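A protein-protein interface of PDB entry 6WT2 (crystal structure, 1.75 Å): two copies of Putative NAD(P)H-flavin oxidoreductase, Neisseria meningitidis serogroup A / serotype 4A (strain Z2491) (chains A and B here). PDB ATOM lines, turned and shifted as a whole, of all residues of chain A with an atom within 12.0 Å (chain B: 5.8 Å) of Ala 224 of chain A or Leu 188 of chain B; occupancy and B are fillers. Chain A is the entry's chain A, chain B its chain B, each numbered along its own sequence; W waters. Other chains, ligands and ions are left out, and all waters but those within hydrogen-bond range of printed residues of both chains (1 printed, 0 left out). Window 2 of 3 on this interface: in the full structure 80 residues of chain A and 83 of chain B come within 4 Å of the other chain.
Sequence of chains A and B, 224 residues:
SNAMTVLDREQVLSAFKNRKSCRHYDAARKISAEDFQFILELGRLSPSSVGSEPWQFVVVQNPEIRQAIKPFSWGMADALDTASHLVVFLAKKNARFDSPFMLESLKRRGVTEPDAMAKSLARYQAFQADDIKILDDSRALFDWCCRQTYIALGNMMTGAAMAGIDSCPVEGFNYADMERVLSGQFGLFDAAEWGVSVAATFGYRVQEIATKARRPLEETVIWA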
ATOM      1  N   LEU A 217      11.886 -15.444  -1.361  1.00  0.00           N
ATOM      2  CA  LEU A 217      11.257 -16.504  -2.135  1.00  0.00           C
ATOM      3  C   LEU A 217      12.027 -16.805  -3.417  1.00  0.00           C
ATOM      4  O   LEU A 217      12.111 -17.963  -3.835  1.00  0.00           O
ATOM      5  CB  LEU A 217       9.811 -16.107  -2.435  1.00  0.00           C
ATOM      6  CG  LEU A 217       8.727 -17.158  -2.683  1.00  0.00           C
ATOM      7  CD1 LEU A 217       8.659 -18.182  -1.566  1.00  0.00           C
ATOM      8  CD2 LEU A 217       7.377 -16.465  -2.866  1.00  0.00           C
ATOM      9  N   GLU A 218      12.646 -15.787  -4.028  1.00  0.00           N
ATOM     10  CA  GLU A 218      13.388 -15.994  -5.261  1.00  0.00           C
ATOM     11  C   GLU A 218      14.643 -16.838  -5.056  1.00  0.00           C
ATOM     12  O   GLU A 218      15.227 -17.309  -6.037  1.00  0.00           O
ATOM     13  CB  GLU A 218      13.751 -14.636  -5.878  1.00  0.00           C
ATOM     14  CG  GLU A 218      12.544 -13.760  -6.278  1.00  0.00           C
ATOM     15  CD  GLU A 218      11.633 -13.367  -5.103  1.00  0.00           C
ATOM     16  OE1 GLU A 218      10.389 -13.385  -5.283  1.00  0.00           O
ATOM     17  OE2 GLU A 218      12.151 -13.064  -3.999  1.00  0.00           O
ATOM     18  N   GLU A 219      15.089 -17.021  -3.815  1.00  0.00           N
ATOM     19  CA  GLU A 219      16.191 -17.921  -3.498  1.00  0.00           C
ATOM     20  C   GLU A 219      15.702 -19.269  -2.969  1.00  0.00           C
ATOM     21  O   GLU A 219      16.491 -20.037  -2.410  1.00  0.00           O
ATOM     22  CB  GLU A 219      17.126 -17.268  -2.478  1.00  0.00           C
ATOM     23  CG  GLU A 219      17.761 -15.968  -2.964  1.00  0.00           C
ATOM     24  CD  GLU A 219      18.553 -15.256  -1.872  1.00  0.00           C
ATOM     25  OE1 GLU A 219      19.274 -15.938  -1.110  1.00  0.00           O
ATOM     26  OE2 GLU A 219      18.445 -14.014  -1.766  1.00  0.00           O
ATOM     27  N   THR A 220      14.423 -19.563  -3.118  1.00  0.00           N
ATOM     28  CA  THR A 220      13.892 -20.805  -2.563  1.00  0.00           C
ATOM     29  C   THR A 220      13.078 -21.532  -3.616  1.00  0.00           C
ATOM     30  O   THR A 220      13.059 -22.764  -3.653  1.00  0.00           O
ATOM     31  CB  THR A 220      13.058 -20.507  -1.320  1.00  0.00           C
ATOM     32  OG1 THR A 220      13.941 -20.151  -0.243  1.00  0.00           O
ATOM     33  CG2 THR A 220      12.217 -21.723  -0.914  1.00  0.00           C
ATOM     34  N   VAL A 221      12.422 -20.776  -4.492  1.00  0.00           N
ATOM     35  CA  VAL A 221      11.509 -21.346  -5.470  1.00  0.00           C
ATOM     36  C   VAL A 221      12.258 -21.569  -6.771  1.00  0.00           C
ATOM     37  O   VAL A 221      12.962 -20.670  -7.263  1.00  0.00           O
ATOM     38  CB  VAL A 221      10.280 -20.444  -5.683  1.00  0.00           C
ATOM     39  CG1 VAL A 221       9.353 -21.045  -6.765  1.00  0.00           C
ATOM     40  CG2 VAL A 221       9.535 -20.282  -4.370  1.00  0.00           C
ATOM     41  N   ILE A 222      12.105 -22.763  -7.331  1.00  0.00           N
ATOM     42  CA  ILE A 222      12.658 -23.107  -8.631  1.00  0.00           C
ATOM     43  C   ILE A 222      11.486 -23.361  -9.564  1.00  0.00           C
ATOM     44  O   ILE A 222      10.737 -24.324  -9.381  1.00  0.00           O
ATOM     45  CB  ILE A 222      13.584 -24.324  -8.565  1.00  0.00           C
ATOM     46  CG1 ILE A 222      14.724 -24.056  -7.584  1.00  0.00           C
ATOM     47  CG2 ILE A 222      14.121 -24.644  -9.964  1.00  0.00           C
ATOM     48  CD1 ILE A 222      15.679 -25.207  -7.440  1.00  0.00           C
ATOM     49  N   TRP A 223      11.330 -22.499 -10.564  1.00  0.00           N
ATOM     50  CA  TRP A 223      10.207 -22.584 -11.487  1.00  0.00           C
ATOM     51  C   TRP A 223      10.556 -23.521 -12.633  1.00  0.00           C
ATOM     52  O   TRP A 223      11.528 -23.293 -13.356  1.00  0.00           O
ATOM     53  CB  TRP A 223       9.840 -21.194 -12.006  1.00  0.00           C
ATOM     54  CG  TRP A 223       9.148 -20.380 -10.957  1.00  0.00           C
ATOM     55  CD1 TRP A 223       9.702 -19.418 -10.160  1.00  0.00           C
ATOM     56  CD2 TRP A 223       7.775 -20.485 -10.568  1.00  0.00           C
ATOM     57  NE1 TRP A 223       8.751 -18.911  -9.308  1.00  0.00           N
ATOM     58  CE2 TRP A 223       7.559 -19.542  -9.544  1.00  0.00           C
ATOM     59  CE3 TRP A 223       6.703 -21.281 -10.992  1.00  0.00           C
ATOM     60  CZ2 TRP A 223       6.314 -19.379  -8.931  1.00  0.00           C
ATOM     61  CZ3 TRP A 223       5.471 -21.109 -10.395  1.00  0.00           C
ATOM     62  CH2 TRP A 223       5.287 -20.168  -9.371  1.00  0.00           C
ATOM     63  N   ALA A 224       9.757 -24.565 -12.796  1.00  0.00           N
ATOM     64  CA  ALA A 224       9.955 -25.537 -13.863  1.00  0.00           C
ATOM     65  C   ALA A 224       8.596 -26.079 -14.286  1.00  0.00           C
ATOM     66  O   ALA A 224       8.461 -27.226 -14.712  1.00  0.00           O
ATOM     67  CB  ALA A 224      10.862 -26.660 -13.406  1.00  0.00           C
ATOM     68  OXT ALA A 224       7.591 -25.377 -14.181  1.00  0.00           O
ATOM     69  N   VAL B  58      10.597 -26.837  -5.786  1.00  0.00           N
ATOM     70  CA  VAL B  58      10.613 -26.969  -7.243  1.00  0.00           C
ATOM     71  C   VAL B  58       9.171 -27.027  -7.712  1.00  0.00           C
ATOM     72  O   VAL B  58       8.460 -27.993  -7.428  1.00  0.00           O
ATOM     73  CB  VAL B  58      11.371 -28.217  -7.705  1.00  0.00           C
ATOM     74  CG1 VAL B  58      11.346 -28.290  -9.218  1.00  0.00           C
ATOM     75  CG2 VAL B  58      12.789 -28.234  -7.153  1.00  0.00           C
ATOM     76  N   VAL B  59       8.733 -25.998  -8.422  1.00  0.00           N
ATOM     77  CA  VAL B  59       7.373 -25.950  -8.945  1.00  0.00           C
ATOM     78  C   VAL B  59       7.400 -26.525 -10.356  1.00  0.00           C
ATOM     79  O   VAL B  59       8.009 -25.948 -11.259  1.00  0.00           O
ATOM     80  CB  VAL B  59       6.819 -24.524  -8.928  1.00  0.00           C
ATOM     81  CG1 VAL B  59       5.343 -24.531  -9.255  1.00  0.00           C
ATOM     82  CG2 VAL B  59       7.056 -23.900  -7.575  1.00  0.00           C
ATOM     83  N   VAL B  60       6.748 -27.667 -10.545  1.00  0.00           N
ATOM     84  CA  VAL B  60       6.854 -28.432 -11.782  1.00  0.00           C
ATOM     85  C   VAL B  60       5.573 -28.167 -12.563  1.00  0.00           C
ATOM     86  O   VAL B  60       4.612 -28.922 -12.494  1.00  0.00           O
ATOM     87  CB  VAL B  60       7.077 -29.916 -11.508  1.00  0.00           C
ATOM     88  CG1 VAL B  60       7.175 -30.703 -12.814  1.00  0.00           C
ATOM     89  CG2 VAL B  60       8.325 -30.095 -10.671  1.00  0.00           C
ATOM     90  N   GLN B  61       5.569 -27.079 -13.337  1.00  0.00           N
ATOM     91  CA  GLN B  61       4.436 -26.771 -14.204  1.00  0.00           C
ATOM     92  C   GLN B  61       4.651 -27.203 -15.651  1.00  0.00           C
ATOM     93  O   GLN B  61       3.682 -27.279 -16.412  1.00  0.00           O
ATOM     94  CB  GLN B  61       4.131 -25.268 -14.152  1.00  0.00           C
ATOM     95  CG  GLN B  61       3.838 -24.802 -12.744  1.00  0.00           C
ATOM     96  CD  GLN B  61       2.688 -25.581 -12.151  1.00  0.00           C
ATOM     97  OE1 GLN B  61       2.891 -26.581 -11.458  1.00  0.00           O
ATOM     98  NE2 GLN B  61       1.469 -25.145 -12.445  1.00  0.00           N
ATOM     99  N   ASN B  62       5.871 -27.524 -16.032  1.00  0.00           N
ATOM    100  CA  ASN B  62       6.158 -27.956 -17.393  1.00  0.00           C
ATOM    101  C   ASN B  62       5.574 -29.342 -17.652  1.00  0.00           C
ATOM    102  O   ASN B  62       6.059 -30.320 -17.061  1.00  0.00           O
ATOM    103  CB  ASN B  62       7.666 -27.964 -17.600  1.00  0.00           C
ATOM    104  CG  ASN B  62       8.064 -28.197 -19.038  1.00  0.00           C
ATOM    105  OD1 ASN B  62       7.365 -28.864 -19.805  1.00  0.00           O
ATOM    106  ND2 ASN B  62       9.220 -27.658 -19.408  1.00  0.00           N
ATOM    107  N   ILE B  65       8.016 -32.214 -18.135  1.00  0.00           N
ATOM    108  CA  ILE B  65       8.642 -32.803 -16.955  1.00  0.00           C
ATOM    109  C   ILE B  65       7.656 -33.710 -16.233  1.00  0.00           C
ATOM    110  O   ILE B  65       8.026 -34.781 -15.742  1.00  0.00           O
ATOM    111  CB  ILE B  65       9.189 -31.699 -16.033  1.00  0.00           C
ATOM    112  CG1 ILE B  65      10.192 -30.823 -16.803  1.00  0.00           C
ATOM    113  CG2 ILE B  65       9.841 -32.327 -14.811  1.00  0.00           C
ATOM    114  CD1 ILE B  65      10.802 -29.676 -15.967  1.00  0.00           C
ATOM    115  N   LEU B 182      14.942 -34.781 -12.561  1.00  0.00           N
ATOM    116  CA  LEU B 182      14.856 -33.353 -12.259  1.00  0.00           C
ATOM    117  C   LEU B 182      16.224 -32.682 -12.313  1.00  0.00           C
ATOM    118  O   LEU B 182      16.353 -31.560 -12.819  1.00  0.00           O
ATOM    119  CB  LEU B 182      14.229 -33.136 -10.881  1.00  0.00           C
ATOM    120  CG  LEU B 182      12.779 -33.546 -10.675  1.00  0.00           C
ATOM    121  CD1 LEU B 182      12.360 -33.217  -9.238  1.00  0.00           C
ATOM    122  CD2 LEU B 182      11.848 -32.879 -11.672  1.00  0.00           C
ATOM    123  N   SER B 183      17.256 -33.351 -11.803  1.00  0.00           N
ATOM    124  CA  SER B 183      18.584 -32.755 -11.744  1.00  0.00           C
ATOM    125  C   SER B 183      19.432 -33.073 -12.969  1.00  0.00           C
ATOM    126  O   SER B 183      20.167 -32.207 -13.451  1.00  0.00           O
ATOM    127  CB  SER B 183      19.315 -33.232 -10.492  1.00  0.00           C
ATOM    128  OG  SER B 183      20.698 -33.056 -10.671  1.00  0.00           O
ATOM    129  N   GLY B 184      19.376 -34.303 -13.465  1.00  0.00           N
ATOM    130  CA  GLY B 184      20.236 -34.685 -14.567  1.00  0.00           C
ATOM    131  C   GLY B 184      19.636 -34.311 -15.901  1.00  0.00           C
ATOM    132  O   GLY B 184      20.220 -33.530 -16.658  1.00  0.00           O
ATOM    133  N   PHE B 186      16.839 -32.531 -16.650  1.00  0.00           N
ATOM    134  CA  PHE B 186      16.352 -31.165 -16.803  1.00  0.00           C
ATOM    135  C   PHE B 186      17.208 -30.124 -16.091  1.00  0.00           C
ATOM    136  O   PHE B 186      16.926 -28.923 -16.213  1.00  0.00           O
ATOM    137  CB  PHE B 186      14.893 -31.084 -16.349  1.00  0.00           C
ATOM    138  CG  PHE B 186      13.952 -31.817 -17.266  1.00  0.00           C
ATOM    139  CD1 PHE B 186      13.638 -31.294 -18.515  1.00  0.00           C
ATOM    140  CD2 PHE B 186      13.406 -33.038 -16.900  1.00  0.00           C
ATOM    141  CE1 PHE B 186      12.794 -31.965 -19.381  1.00  0.00           C
ATOM    142  CE2 PHE B 186      12.557 -33.716 -17.754  1.00  0.00           C
ATOM    143  CZ  PHE B 186      12.241 -33.187 -18.984  1.00  0.00           C
ATOM    144  N   GLY B 187      18.250 -30.542 -15.375  1.00  0.00           N
ATOM    145  CA  GLY B 187      19.215 -29.594 -14.842  1.00  0.00           C
ATOM    146  C   GLY B 187      18.638 -28.567 -13.895  1.00  0.00           C
ATOM    147  O   GLY B 187      19.108 -27.422 -13.876  1.00  0.00           O
ATOM    148  N   LEU B 188      17.654 -28.949 -13.085  1.00  0.00           N
ATOM    149  CA  LEU B 188      16.939 -27.987 -12.254  1.00  0.00           C
ATOM    150  C   LEU B 188      17.655 -27.671 -10.954  1.00  0.00           C
ATOM    151  O   LEU B 188      17.373 -26.626 -10.359  1.00  0.00           O
ATOM    152  CB  LEU B 188      15.539 -28.500 -11.922  1.00  0.00           C
ATOM    153  CG  LEU B 188      14.640 -28.821 -13.113  1.00  0.00           C
ATOM    154  CD1 LEU B 188      13.324 -29.384 -12.594  1.00  0.00           C
ATOM    155  CD2 LEU B 188      14.410 -27.587 -13.934  1.00  0.00           C
ATOM    156  N   PHE B 189      18.544 -28.549 -10.492  1.00  0.00           N
ATOM    157  CA  PHE B 189      19.295 -28.295  -9.271  1.00  0.00           C
ATOM    158  C   PHE B 189      20.553 -29.149  -9.277  1.00  0.00           C
ATOM    159  O   PHE B 189      20.663 -30.128 -10.018  1.00  0.00           O
ATOM    160  CB  PHE B 189      18.443 -28.559  -8.014  1.00  0.00           C
ATOM    161  CG  PHE B 189      18.016 -30.000  -7.830  1.00  0.00           C
ATOM    162  CD1 PHE B 189      18.791 -30.884  -7.093  1.00  0.00           C
ATOM    163  CD2 PHE B 189      16.819 -30.461  -8.371  1.00  0.00           C
ATOM    164  CE1 PHE B 189      18.392 -32.209  -6.918  1.00  0.00           C
ATOM    165  CE2 PHE B 189      16.414 -31.779  -8.199  1.00  0.00           C
ATOM    166  CZ  PHE B 189      17.198 -32.658  -7.476  1.00  0.00           C
ATOM    167  N   ASP B 190      21.514 -28.740  -8.456  1.00  0.00           N
ATOM    168  CA  ASP B 190      22.761 -29.473  -8.264  1.00  0.00           C
ATOM    169  C   ASP B 190      22.511 -30.578  -7.244  1.00  0.00           C
ATOM    170  O   ASP B 190      22.381 -30.307  -6.045  1.00  0.00           O
ATOM    171  CB  ASP B 190      23.856 -28.511  -7.808  1.00  0.00           C
ATOM    172  CG  ASP B 190      25.227 -29.161  -7.716  1.00  0.00           C
ATOM    173  OD1 ASP B 190      25.345 -30.385  -7.933  1.00  0.00           O
ATOM    174  OD2 ASP B 190      26.198 -28.435  -7.419  1.00  0.00           O
HETATM  175  O   HOH W   1      10.465 -26.308 -17.144  1.00  0.00           O
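The backbone carbonyl oxygen of Ile 222 of chain A lies within hydrogen-bond range of the backbone NH of Val 59 of chain B (2.8 Å).
O of Val 59 of chain B lies within hydrogen-bond range of N of Ala 224 of chain A, 2.7 Å away.
OXT of Ala 224 of chain A sits at hydrogen-bond distance from N of Gln 61 of chain B (2.8 Å).
N of Asn 62 of chain B is in hydrogen-bond range of O of Ala 224 of chain A, 2.9 Å away.
N of Leu 188 of chain B lies within hydrogen-bond range of O of Leu 182 of chain B.
Among the printed residues, pairs that only touch across the chains: Val 221 of chain A with Val 59 of chain B (3.8 Å), Ile 222 of chain A with Val 58 of chain B (3.4 Å), Ile 222 of chain A with Leu 188 of chain B (3.7 Å), Trp 223 of chain A with Val 59 of chain B (3.6 Å), Ala 224 of chain A with Val 60 of chain B (3.6 Å), Ala 224 of chain A with Ile 65 of chain B (3.6 Å) and Ala 224 of chain A with Leu 188 of chain B (3.7 Å).
Ala 224 of chain A touches six residues of chain B.
Of chain A, only Ile 222 and Ala 224 come within 4 Å of Leu 188 of chain B.
Val 60 of chain B touches one residue of chain A.
Of chain A, only Ala 224 comes within 4 Å of Gln 61 of chain B.
Asn 62 of chain B touches just one residue of chain A: Ala 224 (2.9 Å).
Ile 65 of chain B touches just one residue of chain A: Ala 224.
No residue of chain A comes within 4 Å of Ser 183 of chain B.
Phe 186 of chain B touches none of the printed residues of chain A.
No residue of chain A comes within 4 Å of Gly 187 of chain B.
Printed residues of chain B within 4 Å of Val 221 of chain A: Val 59.
Printed residues of chain B within 4 Å of Trp 223 of chain A: Val 59 (3.6 Å).
Of the printed residues of chain B, Ile 222 of chain A touches Val 58 (3.4 Å), Val 59 (2.8 Å) and Leu 188 (3.7 Å).
Glu 219 of chain A touches none of the printed residues of chain B.
Glu 218 of chain A touches none of the printed residues of chain B.
The nearest printed residue of chain B that does not touch Ile 222 of chain A is Phe 189 of chain B (4.4 Å).
Hydrophobic or aromatic side chains of chain B within 4 Å of the printed part of chain A: Val 59, Ile 65 and Leu 188.
Hydrophobic or aromatic side chains of chain A that line the printed part of chain B: Val 221, Ile 222, Trp 223 and Ala 224.
Along chain A the printed residues that touch a printed residue of chain B span positions 221 to 224.
Among the printed residues, 11 pairs touch across the chains.
No position is printed for both chains.
Water W1 lies within hydrogen-bond range of ND2 of Asn 62 of chain B and O of Ala 224 of chain A.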
